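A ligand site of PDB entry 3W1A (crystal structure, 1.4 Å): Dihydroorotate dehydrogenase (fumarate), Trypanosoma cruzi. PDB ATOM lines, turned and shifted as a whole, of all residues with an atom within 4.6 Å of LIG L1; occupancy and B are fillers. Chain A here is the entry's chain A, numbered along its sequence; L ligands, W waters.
An oxygen (O8) of LIG L1 lies within hydrogen-bond range of the backbone NH (N) of Thr 273. OG1 of Thr 273 sits at hydrogen-bond distance from O8 of LIG L1. The backbone NH (N) of Gly 223 lies within hydrogen-bond range of an oxygen (O7) of LIG L1, 2.7 Å away. N of Ser 45 is in hydrogen-bond range of O2 of LIG L1, at 3.3 Å. OG of Ser 45 sits at hydrogen-bond distance from N2 of LIG L1 (2.8 Å). The backbone NH (N) of Gly 251 lies within hydrogen-bond range of an oxygen (O7) of LIG L1 (2.8 Å). NZ of Lys 44 is in hydrogen-bond range of O2 of LIG L1, 2.8 Å away. An oxygen (O3) of LIG L1 sits at hydrogen-bond distance from the backbone carbonyl oxygen (O) of Ala 20, at 2.8 Å. O of Val 194 sits at hydrogen-bond distance from O4 of LIG L1 (2.8 Å). O9 of LIG L1 is in hydrogen-bond range of N of Gly 272 (2.9 Å). The side-chain amino group of Lys 165 lies within hydrogen-bond range of an oxygen (O3) of LIG L1, at 2.9 Å. The side-chain amide nitrogen of Asn 195 is in hydrogen-bond range of an oxygen (O1) of LIG L1. ND2 of Asn 128 sits at hydrogen-bond distance from O1 of LIG L1, at 3.3 Å. The side-chain sulfur of Cys 249 is in hydrogen-bond range of an oxygen (O4) of LIG L1, at 3.5 Å. An oxygen (O4) of LG2 L2 is in salt-bridge range of the side-chain amino group of Lys 44. The side-chain amide oxygen of Asn 195 is in hydrogen-bond range of a nitrogen (N2) of LG2 L2 (2.7 Å). ND2 of Asn 128 is in hydrogen-bond range of O2 of LG2 L2 (2.9 Å). OD1 of Asn 68 sits at hydrogen-bond distance from N1 of LG2 L2. OG of Ser 196 is in hydrogen-bond range of O1 of LG2 L2 (2.8 Å). O3 of LG2 L2 sits at hydrogen-bond distance from N of Met 70 (3.1 Å). The backbone NH (N) of Leu 72 is in hydrogen-bond range of an oxygen (O4) of LG2 L2 (2.8 Å).
A nitrogen (N1) of LIG L1 lies close to a nitrogen (N2) of LG2 L2.
OG of Ser 66 sits at hydrogen-bond distance from OG1 of Thr 273 (2.7 Å). OG of Ser 45 sits at hydrogen-bond distance from ND2 of Asn 128 (3.1 Å). OG of Ser 45 lies within hydrogen-bond range of OG of Ser 98 (2.6 Å). N of Val 194 is in hydrogen-bond range of O of Cys 249, at 2.9 Å. OD1 of Asn 128 is in hydrogen-bond range of ND2 of Asn 195 (3.3 Å). O of Val 271 sits at hydrogen-bond distance from N of Ala 19 (2.9 Å). OD1 of Asn 68 lies within hydrogen-bond range of N of Met 70 (3.3 Å). O of Gly 222 is in hydrogen-bond range of N of Ser 66, 2.9 Å away.
Ala 19 touches LIG L1. Gly 21 touches LIG L1 (CA to N3, 3.2 Å). Tyr 59 touches LIG L1. Asn 68 touches LIG L1. CG of Met 70 touches C7 of LIG L1, 3.8 Å away. Ser 196 touches LIG L1. Gly 222 touches LIG L1 (CA to O7, 3.6 Å). Ile 226 touches LIG L1 (CD1 to O7, 3.7 Å). Gly 250 touches LIG L1. Hydrophobic or aromatic side chains within 4 Å of LIG L1: Ala 19, Ala 20, Tyr 59, Met 70 and Ile 226. Within 4 Å of LIG L1: Ala 19, Ala 20, Gly 21, Lys 44, Ser 45, Tyr 59, Asn 68, Met 70, Asn 128, Lys 165, Val 194, Asn 195, Ser 196, Gly 222, Gly 223, Ile 226, Cys 249, Gly 250, Gly 251, Gly 272 and Thr 273. The nearest printed residue that does not touch LIG L1 is Val 22 (4.003 Å).
Water W4 lies within hydrogen-bond range of an oxygen (O5) of LIG L1 (2.7 Å) and the side-chain amide nitrogen of Asn 68 (3.2 Å). Water W3 bridges O9 of LIG L1 and O of Val 252. Water W2 lies within hydrogen-bond range of OG of Ser 98, OE1 of Glu 126 and O1 of LIG L1.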
ATOM      1  N   ALA A  19       5.791 -21.668  33.565  1.00  0.00           N
ATOM      2  CA  ALA A  19       5.355 -21.425  32.211  1.00  0.00           C
ATOM      3  C   ALA A  19       6.005 -20.180  31.650  1.00  0.00           C
ATOM      4  O   ALA A  19       6.235 -19.221  32.393  1.00  0.00           O
ATOM      5  CB  ALA A  19       3.828 -21.269  32.179  1.00  0.00           C
ATOM      6  N   ALA A  20       6.358 -20.162  30.375  1.00  0.00           N
ATOM      7  CA  ALA A  20       7.014 -18.980  29.826  1.00  0.00           C
ATOM      8  C   ALA A  20       6.222 -17.729  30.102  1.00  0.00           C
ATOM      9  O   ALA A  20       4.935 -17.714  30.051  1.00  0.00           O
ATOM     10  CB  ALA A  20       7.214 -19.149  28.337  1.00  0.00           C
ATOM     11  N   GLY A  21       6.892 -16.635  30.437  1.00  0.00           N
ATOM     12  CA  GLY A  21       6.216 -15.390  30.768  1.00  0.00           C
ATOM     13  C   GLY A  21       6.041 -15.128  32.241  1.00  0.00           C
ATOM     14  O   GLY A  21       5.875 -13.972  32.621  1.00  0.00           O
ATOM     15  N   VAL A  22       5.987 -16.197  33.050  1.00  0.00           N
ATOM     16  CA  VAL A  22       5.707 -16.007  34.471  1.00  0.00           C
ATOM     17  C   VAL A  22       7.019 -16.109  35.244  1.00  0.00           C
ATOM     18  O   VAL A  22       7.730 -17.116  35.101  1.00  0.00           O
ATOM     19  CB  VAL A  22       4.640 -17.019  34.971  1.00  0.00           C
ATOM     20  CG1 VAL A  22       4.459 -16.865  36.495  1.00  0.00           C
ATOM     21  CG2 VAL A  22       3.309 -16.781  34.233  1.00  0.00           C
ATOM     22  N   LYS A  44      11.237 -15.512  29.634  1.00  0.00           N
ATOM     23  CA  LYS A  44      10.108 -14.784  28.985  1.00  0.00           C
ATOM     24  C   LYS A  44      10.296 -14.827  27.472  1.00  0.00           C
ATOM     25  O   LYS A  44      11.411 -14.568  26.960  1.00  0.00           O
ATOM     26  CB  LYS A  44      10.190 -13.317  29.445  1.00  0.00           C
ATOM     27  CG  LYS A  44       9.307 -12.309  28.641  1.00  0.00           C
ATOM     28  CD  LYS A  44       7.817 -12.651  28.879  1.00  0.00           C
ATOM     29  CE  LYS A  44       6.960 -11.898  27.827  1.00  0.00           C
ATOM     30  NZ  LYS A  44       5.505 -12.257  28.134  1.00  0.00           N
ATOM     31  N   SER A  45       9.207 -15.035  26.709  1.00  0.00           N
ATOM     32  CA  SER A  45       9.327 -15.018  25.242  1.00  0.00           C
ATOM     33  C   SER A  45       9.909 -13.687  24.798  1.00  0.00           C
ATOM     34  O   SER A  45       9.418 -12.603  25.252  1.00  0.00           O
ATOM     35  CB  SER A  45       7.977 -15.138  24.555  1.00  0.00           C
ATOM     36  OG  SER A  45       7.537 -16.520  24.703  1.00  0.00           O
ATOM     37  N   TYR A  59      -2.809  -7.531  33.233  1.00  0.00           N
ATOM     38  CA  TYR A  59      -2.929  -8.853  33.837  1.00  0.00           C
ATOM     39  C   TYR A  59      -3.881  -8.708  34.971  1.00  0.00           C
ATOM     40  O   TYR A  59      -3.722  -7.775  35.802  1.00  0.00           O
ATOM     41  CB  TYR A  59      -1.584  -9.343  34.345  1.00  0.00           C
ATOM     42  CG  TYR A  59      -1.724 -10.602  35.220  1.00  0.00           C
ATOM     43  CD1 TYR A  59      -1.808 -10.527  36.623  1.00  0.00           C
ATOM     44  CD2 TYR A  59      -1.761 -11.856  34.613  1.00  0.00           C
ATOM     45  CE1 TYR A  59      -1.964 -11.708  37.411  1.00  0.00           C
ATOM     46  CE2 TYR A  59      -1.910 -13.051  35.383  1.00  0.00           C
ATOM     47  CZ  TYR A  59      -1.989 -12.919  36.766  1.00  0.00           C
ATOM     48  OH  TYR A  59      -2.129 -14.056  37.496  1.00  0.00           O
ATOM     49  N   SER A  66      -6.820 -16.450  35.295  1.00  0.00           N
ATOM     50  CA  SER A  66      -6.271 -15.135  34.956  1.00  0.00           C
ATOM     51  C   SER A  66      -6.578 -14.750  33.526  1.00  0.00           C
ATOM     52  O   SER A  66      -6.907 -15.623  32.658  1.00  0.00           O
ATOM     53  CB  SER A  66      -4.748 -15.085  35.149  1.00  0.00           C
ATOM     54  OG  SER A  66      -4.095 -15.965  34.215  1.00  0.00           O
ATOM     55  N   ASN A  68      -4.722 -12.092  30.526  1.00  0.00           N
ATOM     56  CA  ASN A  68      -3.576 -11.250  30.270  1.00  0.00           C
ATOM     57  C   ASN A  68      -3.513 -10.843  28.857  1.00  0.00           C
ATOM     58  O   ASN A  68      -3.795 -11.594  27.906  1.00  0.00           O
ATOM     59  CB  ASN A  68      -2.198 -11.912  30.686  1.00  0.00           C
ATOM     60  CG  ASN A  68      -1.613 -12.781  29.604  1.00  0.00           C
ATOM     61  OD1 ASN A  68      -0.887 -12.281  28.710  1.00  0.00           O
ATOM     62  ND2 ASN A  68      -1.915 -14.093  29.647  1.00  0.00           N
ATOM     63  N   MET A  70      -0.305  -9.116  27.907  1.00  0.00           N
ATOM     64  CA  MET A  70       0.982  -8.437  28.235  1.00  0.00           C
ATOM     65  C   MET A  70       1.577  -7.748  27.004  1.00  0.00           C
ATOM     66  O   MET A  70       2.066  -6.592  27.136  1.00  0.00           O
ATOM     67  CB  MET A  70       2.033  -9.414  28.809  1.00  0.00           C
ATOM     68  CG  MET A  70       1.548 -10.268  29.994  1.00  0.00           C
ATOM     69  SD  MET A  70       0.902  -9.307  31.399  1.00  0.00           S
ATOM     70  CE  MET A  70       2.405  -8.675  32.030  1.00  0.00           C
ATOM     71  N   LEU A  72       4.059  -9.149  24.955  1.00  0.00           N
ATOM     72  CA  LEU A  72       5.517  -9.532  24.872  1.00  0.00           C
ATOM     73  C   LEU A  72       6.428  -8.383  25.411  1.00  0.00           C
ATOM     74  O   LEU A  72       7.451  -8.080  24.788  1.00  0.00           O
ATOM     75  CB  LEU A  72       5.925  -9.845  23.449  1.00  0.00           C
ATOM     76  CG  LEU A  72       5.366 -11.186  22.947  1.00  0.00           C
ATOM     77  CD1 LEU A  72       5.608 -11.327  21.405  1.00  0.00           C
ATOM     78  CD2 LEU A  72       6.048 -12.388  23.629  1.00  0.00           C
ATOM     79  N   SER A  98      12.703 -19.054  25.542  1.00  0.00           N
ATOM     80  CA  SER A  98      11.534 -18.918  24.646  1.00  0.00           C
ATOM     81  C   SER A  98      11.741 -17.713  23.694  1.00  0.00           C
ATOM     82  O   SER A  98      12.102 -16.616  24.187  1.00  0.00           O
ATOM     83  CB  SER A  98      10.330 -18.696  25.511  1.00  0.00           C
ATOM     84  OG  SER A  98       9.201 -18.491  24.632  1.00  0.00           O
ATOM     85  N   GLU A 126      12.484 -23.038  23.150  1.00  0.00           N
ATOM     86  CA  GLU A 126      11.020 -23.187  23.002  1.00  0.00           C
ATOM     87  C   GLU A 126      10.529 -22.058  22.065  1.00  0.00           C
ATOM     88  O   GLU A 126      10.645 -20.903  22.414  1.00  0.00           O
ATOM     89  CB  GLU A 126      10.337 -23.209  24.400  1.00  0.00           C
ATOM     90  CG  GLU A 126       8.792 -23.436  24.236  1.00  0.00           C
ATOM     91  CD  GLU A 126       8.161 -23.477  25.615  1.00  0.00           C
ATOM     92  OE1 GLU A 126       7.693 -22.385  26.095  1.00  0.00           O
ATOM     93  OE2 GLU A 126       7.959 -24.558  26.189  1.00  0.00           O
ATOM     94  N   ASN A 128       7.859 -19.990  20.344  1.00  0.00           N
ATOM     95  CA  ASN A 128       6.449 -19.675  20.663  1.00  0.00           C
ATOM     96  C   ASN A 128       5.612 -19.367  19.406  1.00  0.00           C
ATOM     97  O   ASN A 128       5.868 -18.321  18.763  1.00  0.00           O
ATOM     98  CB  ASN A 128       6.462 -18.470  21.623  1.00  0.00           C
ATOM     99  CG  ASN A 128       5.065 -18.049  22.076  1.00  0.00           C
ATOM    100  OD1 ASN A 128       4.053 -18.652  21.693  1.00  0.00           O
ATOM    101  ND2 ASN A 128       5.033 -17.064  22.936  1.00  0.00           N
ATOM    102  N   LYS A 165       5.836 -24.062  21.464  1.00  0.00           N
ATOM    103  CA  LYS A 165       4.687 -23.737  22.370  1.00  0.00           C
ATOM    104  C   LYS A 165       3.418 -23.543  21.493  1.00  0.00           C
ATOM    105  O   LYS A 165       3.383 -22.602  20.625  1.00  0.00           O
ATOM    106  CB  LYS A 165       4.984 -22.416  23.072  1.00  0.00           C
ATOM    107  CG  LYS A 165       3.928 -21.996  24.099  1.00  0.00           C
ATOM    108  CD  LYS A 165       3.845 -22.943  25.320  1.00  0.00           C
ATOM    109  CE  LYS A 165       2.932 -22.316  26.447  1.00  0.00           C
ATOM    110  NZ  LYS A 165       3.590 -21.160  27.115  1.00  0.00           N
ATOM    111  N   VAL A 194      -0.526 -26.155  26.796  1.00  0.00           N
ATOM    112  CA  VAL A 194      -0.955 -25.121  25.853  1.00  0.00           C
ATOM    113  C   VAL A 194      -0.501 -23.739  26.343  1.00  0.00           C
ATOM    114  O   VAL A 194      -0.347 -23.481  27.569  1.00  0.00           O
ATOM    115  CB  VAL A 194      -2.504 -25.154  25.656  1.00  0.00           C
ATOM    116  CG1 VAL A 194      -2.863 -26.448  24.930  1.00  0.00           C
ATOM    117  CG2 VAL A 194      -3.305 -24.928  26.934  1.00  0.00           C
ATOM    118  N   ASN A 195      -0.442 -22.841  25.363  1.00  0.00           N
ATOM    119  CA  ASN A 195      -0.529 -21.386  25.685  1.00  0.00           C
ATOM    120  C   ASN A 195      -1.915 -21.020  26.151  1.00  0.00           C
ATOM    121  O   ASN A 195      -2.844 -21.857  26.249  1.00  0.00           O
ATOM    122  CB  ASN A 195      -0.113 -20.677  24.395  1.00  0.00           C
ATOM    123  CG  ASN A 195       0.570 -19.286  24.637  1.00  0.00           C
ATOM    124  OD1 ASN A 195       0.160 -18.512  25.532  1.00  0.00           O
ATOM    125  ND2 ASN A 195       1.744 -19.081  23.975  1.00  0.00           N
ATOM    126  N   SER A 196      -2.023 -19.725  26.552  1.00  0.00           N
ATOM    127  CA  SER A 196      -3.361 -19.282  27.018  1.00  0.00           C
ATOM    128  C   SER A 196      -4.487 -19.441  26.022  1.00  0.00           C
ATOM    129  O   SER A 196      -4.254 -19.494  24.763  1.00  0.00           O
ATOM    130  CB  SER A 196      -3.276 -17.807  27.488  1.00  0.00           C
ATOM    131  OG  SER A 196      -2.858 -16.974  26.433  1.00  0.00           O
ATOM    132  N   GLY A 222      -5.868 -18.146  31.469  1.00  0.00           N
ATOM    133  CA  GLY A 222      -5.099 -19.242  32.107  1.00  0.00           C
ATOM    134  C   GLY A 222      -5.815 -19.621  33.410  1.00  0.00           C
ATOM    135  O   GLY A 222      -6.797 -18.957  33.867  1.00  0.00           O
ATOM    136  N   GLY A 223      -5.295 -20.727  34.005  1.00  0.00           N
ATOM    137  CA  GLY A 223      -5.768 -21.158  35.310  1.00  0.00           C
ATOM    138  C   GLY A 223      -6.915 -22.178  35.282  1.00  0.00           C
ATOM    139  O   GLY A 223      -6.986 -22.974  34.335  1.00  0.00           O
ATOM    140  N   ILE A 226      -9.042 -23.442  32.224  1.00  0.00           N
ATOM    141  CA  ILE A 226      -8.513 -24.041  31.015  1.00  0.00           C
ATOM    142  C   ILE A 226      -7.985 -25.460  31.237  1.00  0.00           C
ATOM    143  O   ILE A 226      -7.507 -26.056  30.272  1.00  0.00           O
ATOM    144  CB  ILE A 226      -7.402 -23.184  30.311  1.00  0.00           C
ATOM    145  CG1 ILE A 226      -6.051 -23.230  31.010  1.00  0.00           C
ATOM    146  CG2 ILE A 226      -7.868 -21.716  30.163  1.00  0.00           C
ATOM    147  CD1 ILE A 226      -4.933 -22.741  30.108  1.00  0.00           C
ATOM    148  N   CYS A 249       0.953 -27.704  29.995  1.00  0.00           N
ATOM    149  CA  CYS A 249       0.793 -26.384  30.650  1.00  0.00           C
ATOM    150  C   CYS A 249      -0.660 -26.023  30.591  1.00  0.00           C
ATOM    151  O   CYS A 249      -1.279 -26.211  29.551  1.00  0.00           O
ATOM    152  CB  CYS A 249       1.587 -25.369  29.816  1.00  0.00           C
ATOM    153  SG  CYS A 249       1.732 -23.743  30.605  1.00  0.00           S
ATOM    154  N   GLY A 250      -1.211 -25.593  31.746  1.00  0.00           N
ATOM    155  CA  GLY A 250      -2.620 -25.024  31.694  1.00  0.00           C
ATOM    156  C   GLY A 250      -3.333 -25.582  32.908  1.00  0.00           C
ATOM    157  O   GLY A 250      -3.516 -26.815  33.078  1.00  0.00           O
ATOM    158  N   GLY A 251      -3.665 -24.715  33.819  1.00  0.00           N
ATOM    159  CA  GLY A 251      -4.568 -25.076  34.929  1.00  0.00           C
ATOM    160  C   GLY A 251      -3.882 -25.882  36.006  1.00  0.00           C
ATOM    161  O   GLY A 251      -4.627 -26.448  36.855  1.00  0.00           O
ATOM    162  N   VAL A 252      -2.558 -25.838  36.165  1.00  0.00           N
ATOM    163  CA  VAL A 252      -1.967 -26.581  37.303  1.00  0.00           C
ATOM    164  C   VAL A 252      -1.920 -25.722  38.540  1.00  0.00           C
ATOM    165  O   VAL A 252      -1.218 -24.696  38.586  1.00  0.00           O
ATOM    166  CB  VAL A 252      -0.537 -27.028  36.898  1.00  0.00           C
ATOM    167  CG1 VAL A 252       0.128 -27.765  38.103  1.00  0.00           C
ATOM    168  CG2 VAL A 252      -0.650 -28.007  35.730  1.00  0.00           C
ATOM    169  N   VAL A 271       3.829 -24.280  35.007  1.00  0.00           N
ATOM    170  CA  VAL A 271       2.917 -23.648  35.981  1.00  0.00           C
ATOM    171  C   VAL A 271       2.988 -22.157  35.691  1.00  0.00           C
ATOM    172  O   VAL A 271       4.033 -21.511  35.826  1.00  0.00           O
ATOM    173  CB  VAL A 271       3.373 -23.902  37.431  1.00  0.00           C
ATOM    174  CG1 VAL A 271       2.336 -23.393  38.400  1.00  0.00           C
ATOM    175  CG2 VAL A 271       3.544 -25.466  37.609  1.00  0.00           C
ATOM    176  N   GLY A 272       1.803 -21.588  35.278  1.00  0.00           N
ATOM    177  CA  GLY A 272       1.684 -20.189  34.939  1.00  0.00           C
ATOM    178  C   GLY A 272       0.963 -19.434  35.993  1.00  0.00           C
ATOM    179  O   GLY A 272       1.509 -18.939  36.983  1.00  0.00           O
ATOM    180  N   THR A 273      -0.361 -19.249  35.779  1.00  0.00           N
ATOM    181  CA  THR A 273      -1.243 -18.511  36.696  1.00  0.00           C
ATOM    182  C   THR A 273      -0.960 -18.840  38.172  1.00  0.00           C
ATOM    183  O   THR A 273      -0.873 -17.923  39.008  1.00  0.00           O
ATOM    184  CB  THR A 273      -2.757 -18.730  36.303  1.00  0.00           C
ATOM    185  OG1 THR A 273      -2.946 -18.289  34.989  1.00  0.00           O
ATOM    186  CG2 THR A 273      -3.677 -17.994  37.335  1.00  0.00           C
HETATM  187  N1  LIG L   1       3.331 -18.005  27.104  1.00  0.00           N
HETATM  188  C1  LIG L   1       4.452 -17.934  26.361  1.00  0.00           C
HETATM  189  O1  LIG L   1       4.755 -18.929  25.599  1.00  0.00           O
HETATM  190  N2  LIG L   1       5.325 -16.872  26.331  1.00  0.00           N
HETATM  191  C2  LIG L   1       5.109 -15.790  27.110  1.00  0.00           C
HETATM  192  O2  LIG L   1       5.997 -14.856  27.197  1.00  0.00           O
HETATM  193  C3  LIG L   1       3.961 -15.810  27.959  1.00  0.00           C
HETATM  194  N3  LIG L   1       3.759 -14.757  28.803  1.00  0.00           N
HETATM  195  C4  LIG L   1       2.772 -14.908  29.749  1.00  0.00           C
HETATM  196  C5  LIG L   1       2.549 -13.912  30.692  1.00  0.00           C
HETATM  197  C6  LIG L   1       1.538 -14.016  31.663  1.00  0.00           C
HETATM  198  C7  LIG L   1       1.456 -12.916  32.696  1.00  0.00           C
HETATM  199  C8  LIG L   1       0.723 -15.155  31.646  1.00  0.00           C
HETATM  200  C9  LIG L   1      -0.358 -15.307  32.685  1.00  0.00           C
HETATM  201  C10 LIG L   1       0.876 -16.167  30.699  1.00  0.00           C
HETATM  202  C11 LIG L   1       1.921 -16.061  29.745  1.00  0.00           C
HETATM  203  N4  LIG L   1       2.044 -17.017  28.770  1.00  0.00           N
HETATM  204  C12 LIG L   1       3.135 -16.974  27.919  1.00  0.00           C
HETATM  205  C13 LIG L   1       1.197 -18.243  28.757  1.00  0.00           C
HETATM  206  C14 LIG L   1       1.646 -19.221  29.826  1.00  0.00           C
HETATM  207  O3  LIG L   1       2.991 -19.696  29.506  1.00  0.00           O
HETATM  208  C15 LIG L   1       0.742 -20.455  29.883  1.00  0.00           C
HETATM  209  O4  LIG L   1       0.809 -21.081  28.575  1.00  0.00           O
HETATM  210  C16 LIG L   1      -0.745 -20.044  30.174  1.00  0.00           C
HETATM  211  O5  LIG L   1      -0.755 -19.025  31.141  1.00  0.00           O
HETATM  212  C17 LIG L   1      -1.499 -21.275  30.651  1.00  0.00           C
HETATM  213  O6  LIG L   1      -1.007 -21.872  31.837  1.00  0.00           O
HETATM  214  P1  LIG L   1      -1.694 -21.558  33.282  1.00  0.00           P
HETATM  215  O7  LIG L   1      -3.103 -22.075  33.201  1.00  0.00           O
HETATM  216  O8  LIG L   1      -1.664 -20.053  33.485  1.00  0.00           O
HETATM  217  O9  LIG L   1      -0.766 -22.306  34.236  1.00  0.00           O
HETATM  218  C1  LG2 L   2       0.369 -15.113  26.753  1.00  0.00           C
HETATM  219  C2  LG2 L   2       2.076 -15.553  25.170  1.00  0.00           C
HETATM  220  C3  LG2 L   2       2.503 -14.226  25.358  1.00  0.00           C
HETATM  221  O1  LG2 L   2      -0.639 -15.579  27.391  1.00  0.00           O
HETATM  222  N1  LG2 L   2       0.813 -13.868  26.956  1.00  0.00           N
HETATM  223  N2  LG2 L   2       0.978 -15.944  25.829  1.00  0.00           N
HETATM  224  O2  LG2 L   2       2.600 -16.310  24.350  1.00  0.00           O
HETATM  225  F1  LG2 L   2       3.571 -13.832  24.733  1.00  0.00           F
HETATM  226  C4  LG2 L   2       1.862 -13.387  26.284  1.00  0.00           C
HETATM  227  C5  LG2 L   2       2.186 -11.947  26.336  1.00  0.00           C
HETATM  228  O3  LG2 L   2       1.131 -11.246  26.143  1.00  0.00           O
HETATM  229  O4  LG2 L   2       3.335 -11.470  26.392  1.00  0.00           O
HETATM  230  O   HOH W   1      -0.358 -24.927  34.324  1.00  0.00           O
HETATM  231  O   HOH W   2       7.173 -20.120  24.699  1.00  0.00           O
HETATM  232  O   HOH W   3      -1.528 -22.384  36.917  1.00  0.00           O
HETATM  233  O   HOH W   4      -2.576 -17.179  30.382  1.00  0.00           O
